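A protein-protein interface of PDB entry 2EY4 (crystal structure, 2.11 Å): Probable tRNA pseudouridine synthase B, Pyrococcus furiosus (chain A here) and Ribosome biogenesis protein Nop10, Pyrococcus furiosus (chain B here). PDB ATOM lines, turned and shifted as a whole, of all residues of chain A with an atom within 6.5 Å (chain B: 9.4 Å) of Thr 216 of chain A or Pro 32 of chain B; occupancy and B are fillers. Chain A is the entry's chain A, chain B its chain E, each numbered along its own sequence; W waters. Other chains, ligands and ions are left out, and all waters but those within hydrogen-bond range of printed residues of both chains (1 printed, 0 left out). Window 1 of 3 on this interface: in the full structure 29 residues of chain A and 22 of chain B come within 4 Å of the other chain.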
ATOM      1  N   ASN A  50      18.392  17.883   0.234  1.00  0.00           N
ATOM      2  CA  ASN A  50      18.896  18.310  -1.066  1.00  0.00           C
ATOM      3  C   ASN A  50      20.075  19.188  -0.665  1.00  0.00           C
ATOM      4  O   ASN A  50      19.964  20.415  -0.591  1.00  0.00           O
ATOM      5  CB  ASN A  50      17.840  19.131  -1.804  1.00  0.00           C
ATOM      6  CG  ASN A  50      18.269  19.513  -3.212  1.00  0.00           C
ATOM      7  OD1 ASN A  50      17.696  20.421  -3.811  1.00  0.00           O
ATOM      8  ND2 ASN A  50      19.264  18.824  -3.747  1.00  0.00           N
ATOM      9  N   LEU A  51      21.195  18.531  -0.376  1.00  0.00           N
ATOM     10  CA  LEU A  51      22.401  19.209   0.082  1.00  0.00           C
ATOM     11  C   LEU A  51      23.277  19.827  -0.995  1.00  0.00           C
ATOM     12  O   LEU A  51      23.516  19.230  -2.047  1.00  0.00           O
ATOM     13  CB  LEU A  51      23.265  18.240   0.891  1.00  0.00           C
ATOM     14  CG  LEU A  51      24.373  18.912   1.702  1.00  0.00           C
ATOM     15  CD1 LEU A  51      23.776  19.482   2.984  1.00  0.00           C
ATOM     16  CD2 LEU A  51      25.464  17.935   2.037  1.00  0.00           C
ATOM     17  N   ASP A  52      23.767  21.026  -0.715  1.00  0.00           N
ATOM     18  CA  ASP A  52      24.671  21.686  -1.643  1.00  0.00           C
ATOM     19  C   ASP A  52      26.028  21.313  -1.089  1.00  0.00           C
ATOM     20  O   ASP A  52      26.504  21.929  -0.141  1.00  0.00           O
ATOM     21  CB  ASP A  52      24.521  23.206  -1.605  1.00  0.00           C
ATOM     22  CG  ASP A  52      25.290  23.896  -2.733  1.00  0.00           C
ATOM     23  OD1 ASP A  52      26.246  23.290  -3.268  1.00  0.00           O
ATOM     24  OD2 ASP A  52      24.938  25.042  -3.081  1.00  0.00           O
ATOM     25  N   LYS A  53      26.639  20.283  -1.653  1.00  0.00           N
ATOM     26  CA  LYS A  53      27.944  19.842  -1.188  1.00  0.00           C
ATOM     27  C   LYS A  53      29.032  20.897  -1.419  1.00  0.00           C
ATOM     28  O   LYS A  53      29.098  21.506  -2.480  1.00  0.00           O
ATOM     29  CB  LYS A  53      28.349  18.555  -1.899  1.00  0.00           C
ATOM     30  CG  LYS A  53      29.742  18.097  -1.542  1.00  0.00           C
ATOM     31  CD  LYS A  53      30.199  16.927  -2.401  1.00  0.00           C
ATOM     32  CE  LYS A  53      31.621  16.539  -2.053  1.00  0.00           C
ATOM     33  NZ  LYS A  53      32.541  17.682  -2.326  1.00  0.00           N
ATOM     34  N   PRO A  54      29.889  21.126  -0.414  1.00  0.00           N
ATOM     35  CA  PRO A  54      30.972  22.107  -0.539  1.00  0.00           C
ATOM     36  C   PRO A  54      32.220  21.439  -1.106  1.00  0.00           C
ATOM     37  O   PRO A  54      32.407  20.227  -0.956  1.00  0.00           O
ATOM     38  CB  PRO A  54      31.183  22.559   0.895  1.00  0.00           C
ATOM     39  CG  PRO A  54      30.984  21.281   1.651  1.00  0.00           C
ATOM     40  CD  PRO A  54      29.741  20.692   0.989  1.00  0.00           C
ATOM     41  N   PRO A  55      33.071  22.206  -1.804  1.00  0.00           N
ATOM     42  CA  PRO A  55      34.269  21.551  -2.330  1.00  0.00           C
ATOM     43  C   PRO A  55      35.151  21.229  -1.130  1.00  0.00           C
ATOM     44  O   PRO A  55      35.187  21.984  -0.158  1.00  0.00           O
ATOM     45  CB  PRO A  55      34.881  22.618  -3.234  1.00  0.00           C
ATOM     46  CG  PRO A  55      34.488  23.898  -2.560  1.00  0.00           C
ATOM     47  CD  PRO A  55      33.041  23.636  -2.161  1.00  0.00           C
ATOM     48  N   SER A  86      31.386  20.500  -6.146  1.00  0.00           N
ATOM     49  CA  SER A  86      30.335  20.992  -5.271  1.00  0.00           C
ATOM     50  C   SER A  86      28.998  20.730  -5.944  1.00  0.00           C
ATOM     51  O   SER A  86      28.955  20.273  -7.090  1.00  0.00           O
ATOM     52  CB  SER A  86      30.497  22.498  -5.043  1.00  0.00           C
ATOM     53  OG  SER A  86      30.070  23.232  -6.177  1.00  0.00           O
ATOM     54  N   GLY A  87      27.906  20.995  -5.235  1.00  0.00           N
ATOM     55  CA  GLY A  87      26.615  20.807  -5.856  1.00  0.00           C
ATOM     56  C   GLY A  87      25.623  19.842  -5.243  1.00  0.00           C
ATOM     57  O   GLY A  87      25.836  19.283  -4.168  1.00  0.00           O
ATOM     58  N   ARG A 201      30.725  21.570 -10.949  1.00  0.00           N
ATOM     59  CA  ARG A 201      29.626  21.722 -10.003  1.00  0.00           C
ATOM     60  C   ARG A 201      28.355  21.039 -10.530  1.00  0.00           C
ATOM     61  O   ARG A 201      27.970  21.242 -11.680  1.00  0.00           O
ATOM     62  CB  ARG A 201      29.349  23.207  -9.781  1.00  0.00           C
ATOM     63  CG  ARG A 201      28.307  23.497  -8.727  1.00  0.00           C
ATOM     64  CD  ARG A 201      28.122  25.002  -8.550  1.00  0.00           C
ATOM     65  NE  ARG A 201      27.390  25.300  -7.326  1.00  0.00           N
ATOM     66  CZ  ARG A 201      26.112  25.006  -7.133  1.00  0.00           C
ATOM     67  NH1 ARG A 201      25.423  24.416  -8.100  1.00  0.00           N
ATOM     68  NH2 ARG A 201      25.534  25.257  -5.962  1.00  0.00           N
ATOM     69  N   LEU A 214      17.464  23.572  -2.041  1.00  0.00           N
ATOM     70  CA  LEU A 214      18.897  23.298  -1.955  1.00  0.00           C
ATOM     71  C   LEU A 214      19.465  24.009  -0.741  1.00  0.00           C
ATOM     72  O   LEU A 214      19.372  25.231  -0.629  1.00  0.00           O
ATOM     73  CB  LEU A 214      19.619  23.778  -3.213  1.00  0.00           C
ATOM     74  CG  LEU A 214      21.099  23.388  -3.320  1.00  0.00           C
ATOM     75  CD1 LEU A 214      21.236  21.869  -3.463  1.00  0.00           C
ATOM     76  CD2 LEU A 214      21.721  24.085  -4.526  1.00  0.00           C
ATOM     77  N   ILE A 215      20.085  23.254   0.159  1.00  0.00           N
ATOM     78  CA  ILE A 215      20.614  23.846   1.382  1.00  0.00           C
ATOM     79  C   ILE A 215      22.052  23.424   1.706  1.00  0.00           C
ATOM     80  O   ILE A 215      22.468  22.303   1.388  1.00  0.00           O
ATOM     81  CB  ILE A 215      19.669  23.486   2.561  1.00  0.00           C
ATOM     82  CG1 ILE A 215      20.232  24.009   3.877  1.00  0.00           C
ATOM     83  CG2 ILE A 215      19.489  21.974   2.642  1.00  0.00           C
ATOM     84  CD1 ILE A 215      19.333  23.742   5.082  1.00  0.00           C
ATOM     85  N   THR A 216      22.813  24.316   2.339  1.00  0.00           N
ATOM     86  CA  THR A 216      24.200  24.004   2.705  1.00  0.00           C
ATOM     87  C   THR A 216      24.252  23.390   4.099  1.00  0.00           C
ATOM     88  O   THR A 216      23.257  23.391   4.832  1.00  0.00           O
ATOM     89  CB  THR A 216      25.115  25.256   2.760  1.00  0.00           C
ATOM     90  OG1 THR A 216      24.792  26.008   3.935  1.00  0.00           O
ATOM     91  CG2 THR A 216      24.952  26.137   1.508  1.00  0.00           C
ATOM     92  N   LEU A 217      25.426  22.872   4.452  1.00  0.00           N
ATOM     93  CA  LEU A 217      25.658  22.260   5.756  1.00  0.00           C
ATOM     94  C   LEU A 217      25.541  23.309   6.864  1.00  0.00           C
ATOM     95  O   LEU A 217      25.150  22.994   7.994  1.00  0.00           O
ATOM     96  CB  LEU A 217      27.048  21.620   5.796  1.00  0.00           C
ATOM     97  CG  LEU A 217      27.227  20.350   4.963  1.00  0.00           C
ATOM     98  CD1 LEU A 217      28.704  20.108   4.683  1.00  0.00           C
ATOM     99  CD2 LEU A 217      26.600  19.171   5.713  1.00  0.00           C
ATOM    100  N   HIS A 218      25.892  24.551   6.537  1.00  0.00           N
ATOM    101  CA  HIS A 218      25.806  25.641   7.501  1.00  0.00           C
ATOM    102  C   HIS A 218      24.334  25.890   7.816  1.00  0.00           C
ATOM    103  O   HIS A 218      23.956  26.001   8.988  1.00  0.00           O
ATOM    104  CB  HIS A 218      26.467  26.904   6.941  1.00  0.00           C
ATOM    105  CG  HIS A 218      27.936  26.751   6.695  1.00  0.00           C
ATOM    106  ND1 HIS A 218      28.880  26.933   7.684  1.00  0.00           N
ATOM    107  CD2 HIS A 218      28.618  26.359   5.592  1.00  0.00           C
ATOM    108  CE1 HIS A 218      30.080  26.658   7.201  1.00  0.00           C
ATOM    109  NE2 HIS A 218      29.948  26.308   5.934  1.00  0.00           N
ATOM    110  N   ASP A 219      23.505  25.953   6.775  1.00  0.00           N
ATOM    111  CA  ASP A 219      22.076  26.176   6.967  1.00  0.00           C
ATOM    112  C   ASP A 219      21.490  24.990   7.725  1.00  0.00           C
ATOM    113  O   ASP A 219      20.679  25.166   8.640  1.00  0.00           O
ATOM    114  CB  ASP A 219      21.334  26.284   5.630  1.00  0.00           C
ATOM    115  CG  ASP A 219      21.910  27.331   4.704  1.00  0.00           C
ATOM    116  OD1 ASP A 219      22.117  28.477   5.153  1.00  0.00           O
ATOM    117  OD2 ASP A 219      22.136  27.003   3.511  1.00  0.00           O
ATOM    118  N   LEU A 220      21.898  23.783   7.328  1.00  0.00           N
ATOM    119  CA  LEU A 220      21.398  22.566   7.957  1.00  0.00           C
ATOM    120  C   LEU A 220      21.601  22.590   9.463  1.00  0.00           C
ATOM    121  O   LEU A 220      20.638  22.448  10.230  1.00  0.00           O
ATOM    122  CB  LEU A 220      22.080  21.320   7.371  1.00  0.00           C
ATOM    123  CG  LEU A 220      21.514  19.952   7.797  1.00  0.00           C
ATOM    124  CD1 LEU A 220      20.035  19.864   7.455  1.00  0.00           C
ATOM    125  CD2 LEU A 220      22.277  18.834   7.096  1.00  0.00           C
ATOM    126  N   VAL A 221      22.848  22.770   9.890  1.00  0.00           N
ATOM    127  CA  VAL A 221      23.160  22.784  11.310  1.00  0.00           C
ATOM    128  C   VAL A 221      22.414  23.875  12.056  1.00  0.00           C
ATOM    129  O   VAL A 221      21.833  23.619  13.113  1.00  0.00           O
ATOM    130  CB  VAL A 221      24.677  22.942  11.565  1.00  0.00           C
ATOM    131  CG1 VAL A 221      25.419  21.739  11.011  1.00  0.00           C
ATOM    132  CG2 VAL A 221      25.183  24.217  10.929  1.00  0.00           C
ATOM    133  N   ARG B   4      37.161  30.417 -12.121  1.00  0.00           N
ATOM    134  CA  ARG B   4      36.298  30.116 -10.939  1.00  0.00           C
ATOM    135  C   ARG B   4      34.834  30.342 -11.333  1.00  0.00           C
ATOM    136  O   ARG B   4      34.468  31.406 -11.838  1.00  0.00           O
ATOM    137  CB  ARG B   4      36.702  31.015  -9.772  1.00  0.00           C
ATOM    138  CG  ARG B   4      36.262  30.550  -8.411  1.00  0.00           C
ATOM    139  CD  ARG B   4      36.846  29.206  -8.036  1.00  0.00           C
ATOM    140  NE  ARG B   4      36.540  28.896  -6.642  1.00  0.00           N
ATOM    141  CZ  ARG B   4      36.774  27.726  -6.053  1.00  0.00           C
ATOM    142  NH1 ARG B   4      37.322  26.730  -6.737  1.00  0.00           N
ATOM    143  NH2 ARG B   4      36.469  27.555  -4.770  1.00  0.00           N
ATOM    144  N   ILE B   5      34.004  29.331 -11.104  1.00  0.00           N
ATOM    145  CA  ILE B   5      32.599  29.390 -11.471  1.00  0.00           C
ATOM    146  C   ILE B   5      31.779  30.297 -10.571  1.00  0.00           C
ATOM    147  O   ILE B   5      31.863  30.222  -9.352  1.00  0.00           O
ATOM    148  CB  ILE B   5      31.992  27.965 -11.482  1.00  0.00           C
ATOM    149  CG1 ILE B   5      32.765  27.085 -12.475  1.00  0.00           C
ATOM    150  CG2 ILE B   5      30.518  28.028 -11.867  1.00  0.00           C
ATOM    151  CD1 ILE B   5      32.432  25.598 -12.416  1.00  0.00           C
ATOM    152  N   LYS B   7      27.803  32.574 -10.114  1.00  0.00           N
ATOM    153  CA  LYS B   7      26.404  32.615 -10.512  1.00  0.00           C
ATOM    154  C   LYS B   7      25.778  33.865  -9.925  1.00  0.00           C
ATOM    155  O   LYS B   7      26.241  34.385  -8.912  1.00  0.00           O
ATOM    156  CB  LYS B   7      25.651  31.376 -10.033  1.00  0.00           C
ATOM    157  CG  LYS B   7      25.646  31.209  -8.545  1.00  0.00           C
ATOM    158  CD  LYS B   7      24.276  30.779  -8.056  1.00  0.00           C
ATOM    159  CE  LYS B   7      23.849  29.447  -8.631  1.00  0.00           C
ATOM    160  NZ  LYS B   7      22.612  28.989  -7.945  1.00  0.00           N
ATOM    161  N   TYR B  14      24.691  31.259 -14.739  1.00  0.00           N
ATOM    162  CA  TYR B  14      26.068  30.892 -14.426  1.00  0.00           C
ATOM    163  C   TYR B  14      27.017  31.655 -15.346  1.00  0.00           C
ATOM    164  O   TYR B  14      26.779  31.757 -16.548  1.00  0.00           O
ATOM    165  CB  TYR B  14      26.300  29.391 -14.592  1.00  0.00           C
ATOM    166  CG  TYR B  14      26.028  28.585 -13.343  1.00  0.00           C
ATOM    167  CD1 TYR B  14      24.771  28.031 -13.103  1.00  0.00           C
ATOM    168  CD2 TYR B  14      27.027  28.387 -12.394  1.00  0.00           C
ATOM    169  CE1 TYR B  14      24.520  27.293 -11.937  1.00  0.00           C
ATOM    170  CE2 TYR B  14      26.791  27.668 -11.234  1.00  0.00           C
ATOM    171  CZ  TYR B  14      25.534  27.121 -11.010  1.00  0.00           C
ATOM    172  OH  TYR B  14      25.301  26.430  -9.844  1.00  0.00           O
ATOM    173  N   LYS B  28      28.553  35.847  -7.449  1.00  0.00           N
ATOM    174  CA  LYS B  28      29.360  35.266  -6.384  1.00  0.00           C
ATOM    175  C   LYS B  28      29.818  33.867  -6.752  1.00  0.00           C
ATOM    176  O   LYS B  28      29.236  33.220  -7.622  1.00  0.00           O
ATOM    177  CB  LYS B  28      28.563  35.226  -5.074  1.00  0.00           C
ATOM    178  CG  LYS B  28      27.056  35.013  -5.246  1.00  0.00           C
ATOM    179  CD  LYS B  28      26.705  33.652  -5.859  1.00  0.00           C
ATOM    180  CE  LYS B  28      27.016  32.503  -4.899  1.00  0.00           C
ATOM    181  NZ  LYS B  28      26.604  31.172  -5.430  1.00  0.00           N
ATOM    182  N   VAL B  29      30.876  33.408  -6.096  1.00  0.00           N
ATOM    183  CA  VAL B  29      31.389  32.071  -6.353  1.00  0.00           C
ATOM    184  C   VAL B  29      30.235  31.106  -6.069  1.00  0.00           C
ATOM    185  O   VAL B  29      29.630  31.140  -4.999  1.00  0.00           O
ATOM    186  CB  VAL B  29      32.614  31.773  -5.449  1.00  0.00           C
ATOM    187  CG1 VAL B  29      32.992  30.303  -5.532  1.00  0.00           C
ATOM    188  CG2 VAL B  29      33.791  32.636  -5.896  1.00  0.00           C
ATOM    189  N   ALA B  30      29.932  30.259  -7.044  1.00  0.00           N
ATOM    190  CA  ALA B  30      28.828  29.317  -6.929  1.00  0.00           C
ATOM    191  C   ALA B  30      28.958  28.274  -5.822  1.00  0.00           C
ATOM    192  O   ALA B  30      27.951  27.773  -5.312  1.00  0.00           O
ATOM    193  CB  ALA B  30      28.615  28.628  -8.269  1.00  0.00           C
ATOM    194  N   HIS B  31      30.187  27.952  -5.443  1.00  0.00           N
ATOM    195  CA  HIS B  31      30.412  26.952  -4.410  1.00  0.00           C
ATOM    196  C   HIS B  31      30.102  27.499  -3.028  1.00  0.00           C
ATOM    197  O   HIS B  31      30.339  28.678  -2.753  1.00  0.00           O
ATOM    198  CB  HIS B  31      31.861  26.477  -4.463  1.00  0.00           C
ATOM    199  CG  HIS B  31      32.332  26.154  -5.846  1.00  0.00           C
ATOM    200  ND1 HIS B  31      31.920  25.031  -6.530  1.00  0.00           N
ATOM    201  CD2 HIS B  31      33.140  26.836  -6.693  1.00  0.00           C
ATOM    202  CE1 HIS B  31      32.453  25.035  -7.739  1.00  0.00           C
ATOM    203  NE2 HIS B  31      33.197  26.119  -7.865  1.00  0.00           N
ATOM    204  N   PRO B  32      29.535  26.658  -2.146  1.00  0.00           N
ATOM    205  CA  PRO B  32      29.214  27.116  -0.793  1.00  0.00           C
ATOM    206  C   PRO B  32      30.497  27.158   0.028  1.00  0.00           C
ATOM    207  O   PRO B  32      31.477  26.497  -0.310  1.00  0.00           O
ATOM    208  CB  PRO B  32      28.227  26.064  -0.301  1.00  0.00           C
ATOM    209  CG  PRO B  32      28.707  24.826  -0.960  1.00  0.00           C
ATOM    210  CD  PRO B  32      29.004  25.300  -2.375  1.00  0.00           C
ATOM    211  N   PRO B  33      30.506  27.928   1.125  1.00  0.00           N
ATOM    212  CA  PRO B  33      31.701  28.033   1.969  1.00  0.00           C
ATOM    213  C   PRO B  33      32.139  26.701   2.568  1.00  0.00           C
ATOM    214  O   PRO B  33      31.310  25.824   2.836  1.00  0.00           O
ATOM    215  CB  PRO B  33      31.278  29.035   3.033  1.00  0.00           C
ATOM    216  CG  PRO B  33      29.807  28.738   3.195  1.00  0.00           C
ATOM    217  CD  PRO B  33      29.338  28.561   1.769  1.00  0.00           C
ATOM    218  N   ARG B  34      33.445  26.558   2.784  1.00  0.00           N
ATOM    219  CA  ARG B  34      33.985  25.332   3.349  1.00  0.00           C
ATOM    220  C   ARG B  34      33.354  25.054   4.701  1.00  0.00           C
ATOM    221  O   ARG B  34      32.987  25.972   5.425  1.00  0.00           O
ATOM    222  CB  ARG B  34      35.504  25.429   3.498  1.00  0.00           C
ATOM    223  CG  ARG B  34      36.260  25.658   2.186  1.00  0.00           C
ATOM    224  CD  ARG B  34      35.862  24.655   1.105  1.00  0.00           C
ATOM    225  NE  ARG B  34      36.834  24.597   0.014  1.00  0.00           N
ATOM    226  CZ  ARG B  34      37.992  23.943   0.074  1.00  0.00           C
ATOM    227  NH1 ARG B  34      38.331  23.282   1.175  1.00  0.00           N
ATOM    228  NH2 ARG B  34      38.814  23.948  -0.966  1.00  0.00           N
ATOM    229  N   PHE B  35      33.238  23.777   5.043  1.00  0.00           N
ATOM    230  CA  PHE B  35      32.642  23.385   6.310  1.00  0.00           C
ATOM    231  C   PHE B  35      33.550  22.473   7.126  1.00  0.00           C
ATOM    232  O   PHE B  35      34.249  21.616   6.582  1.00  0.00           O
ATOM    233  CB  PHE B  35      31.316  22.666   6.054  1.00  0.00           C
ATOM    234  CG  PHE B  35      30.588  22.267   7.303  1.00  0.00           C
ATOM    235  CD1 PHE B  35      29.821  23.192   8.001  1.00  0.00           C
ATOM    236  CD2 PHE B  35      30.688  20.966   7.797  1.00  0.00           C
ATOM    237  CE1 PHE B  35      29.162  22.828   9.170  1.00  0.00           C
ATOM    238  CE2 PHE B  35      30.035  20.594   8.966  1.00  0.00           C
ATOM    239  CZ  PHE B  35      29.268  21.525   9.658  1.00  0.00           C
ATOM    240  N   ARG B  45      27.407  33.104  14.001  1.00  0.00           N
ATOM    241  CA  ARG B  45      26.555  33.084  12.822  1.00  0.00           C
ATOM    242  C   ARG B  45      25.081  32.971  13.203  1.00  0.00           C
ATOM    243  O   ARG B  45      24.230  33.677  12.665  1.00  0.00           O
ATOM    244  CB  ARG B  45      26.955  31.916  11.918  1.00  0.00           C
ATOM    245  CG  ARG B  45      26.232  31.883  10.582  1.00  0.00           C
ATOM    246  CD  ARG B  45      26.662  30.681   9.737  1.00  0.00           C
ATOM    247  NE  ARG B  45      26.330  29.402  10.368  1.00  0.00           N
ATOM    248  CZ  ARG B  45      27.239  28.519  10.767  1.00  0.00           C
ATOM    249  NH1 ARG B  45      28.533  28.778  10.600  1.00  0.00           N
ATOM    250  NH2 ARG B  45      26.864  27.378  11.323  1.00  0.00           N
ATOM    251  N   LYS B  49      21.835  35.312  12.587  1.00  0.00           N
ATOM    252  CA  LYS B  49      20.809  34.618  11.826  1.00  0.00           C
ATOM    253  C   LYS B  49      19.482  34.596  12.592  1.00  0.00           C
ATOM    254  O   LYS B  49      18.423  34.819  12.006  1.00  0.00           O
ATOM    255  CB  LYS B  49      21.269  33.200  11.479  1.00  0.00           C
ATOM    256  CG  LYS B  49      20.428  32.545  10.391  1.00  0.00           C
ATOM    257  CD  LYS B  49      21.097  31.302   9.801  1.00  0.00           C
ATOM    258  CE  LYS B  49      22.340  31.653   8.998  1.00  0.00           C
ATOM    259  NZ  LYS B  49      22.880  30.458   8.292  1.00  0.00           N
HETATM  260  O   HOH W   1      20.676  29.517   7.035  1.00  0.00           O
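The backbone carbonyl oxygen (O) of Pro 55 of chain A sits close to the guanidinium group (NE) of Arg 34 of chain B (3.1 Å). The side-chain hydroxyl of Ser 86 of chain A lies within hydrogen-bond range of a ring nitrogen (ND1) of His 31 of chain B. NH1 of Arg 201 of chain A sits at hydrogen-bond distance from OH of Tyr 14 of chain B, at 2.7 Å. The guanidinium group (NE) of Arg 201 of chain A lies within hydrogen-bond range of the backbone carbonyl oxygen (O) of Ala 30 of chain B (3.2 Å). A ring nitrogen (NE2) of His 218 of chain A lies within hydrogen-bond range of the backbone carbonyl oxygen of Pro 33 of chain B. NE2 of His 218 of chain A lies within hydrogen-bond range of O of Arg 34 of chain B (3.1 Å). The guanidinium group (NH1) of Arg 45 of chain B is in hydrogen-bond range of a ring nitrogen (ND1) of His 218 of chain A (3.5 Å). OD1 of Asp 219 of chain A is in salt-bridge range of NZ of Lys 49 of chain B (3.8 Å).
Of the 17 printed residues of chain A, 11 touch a printed residue of chain B. Of the 14 printed residues of chain B, 9 touch a printed residue of chain A. Among the printed residues, Asp or Glu carboxylates within 4 Å of a Lys or Arg side-chain nitrogen of the other chain: Asp 219 of chain A with Lys 49 of chain B.
Asp 52 of chain A touches Pro 32 of chain B (OD1 to CD, 3.5 Å). CG of Pro 32 of chain B touches O of Lys 53 of chain A, 3.7 Å away. Pro 54 of chain A touches Pro 32 of chain B. Pro 33 of chain B touches Pro 54 of chain A (O to CB, 3.8 Å). CD of Pro 55 of chain A touches CB of His 31 of chain B (3.8 Å). Pro 55 of chain A touches Pro 32 of chain B (CD to O, 3.7 Å). Pro 32 of chain B touches Thr 216 of chain A (CB to CG2, 3.7 Å). CD1 of Leu 217 of chain A touches CD2 of Phe 35 of chain B, 3.8 Å away. CE1 of His 218 of chain A touches CD1 of Phe 35 of chain B, at 3.6 Å. Val 221 of chain A touches Arg 45 of chain B.
Of chain B, only Pro 32 comes within 4 Å of Asp 52 of chain A. Gly 87 of chain A touches none of the printed residues of chain B. Printed residues of chain B within 4 Å of Leu 217 of chain A: Phe 35. Lys 7 of chain B touches none of the printed residues of chain A. Of the printed residues of chain A, Lys 49 of chain B touches Asp 219.
Water W1 lies within hydrogen-bond range of OD1 of Asp 219 of chain A and NZ of Lys 49 of chain B.
The backbone NH (N) of Gly 87 of chain A is in hydrogen-bond range of the side-chain carboxylate (OD1) of Asp 52 of chain A (3.4 Å). The guanidinium group of Arg 201 of chain A is in salt-bridge range of the side-chain carboxylate of Asp 52 of chain A (2.9 Å). The backbone NH (N) of Asp 52 of chain A is in hydrogen-bond range of the backbone carbonyl oxygen (O) of Ile 215 of chain A (2.8 Å). The backbone carbonyl oxygen of Gly 87 of chain A sits at hydrogen-bond distance from the backbone NH of Lys 53 of chain A, 2.8 Å away. The backbone NH (N) of His 218 of chain A sits close to the side-chain hydroxyl (OG1) of Thr 216 of chain A, 3.2 Å away. O of Ile 5 of chain B sits at hydrogen-bond distance from N of Ala 30 of chain B, 3.0 Å away.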
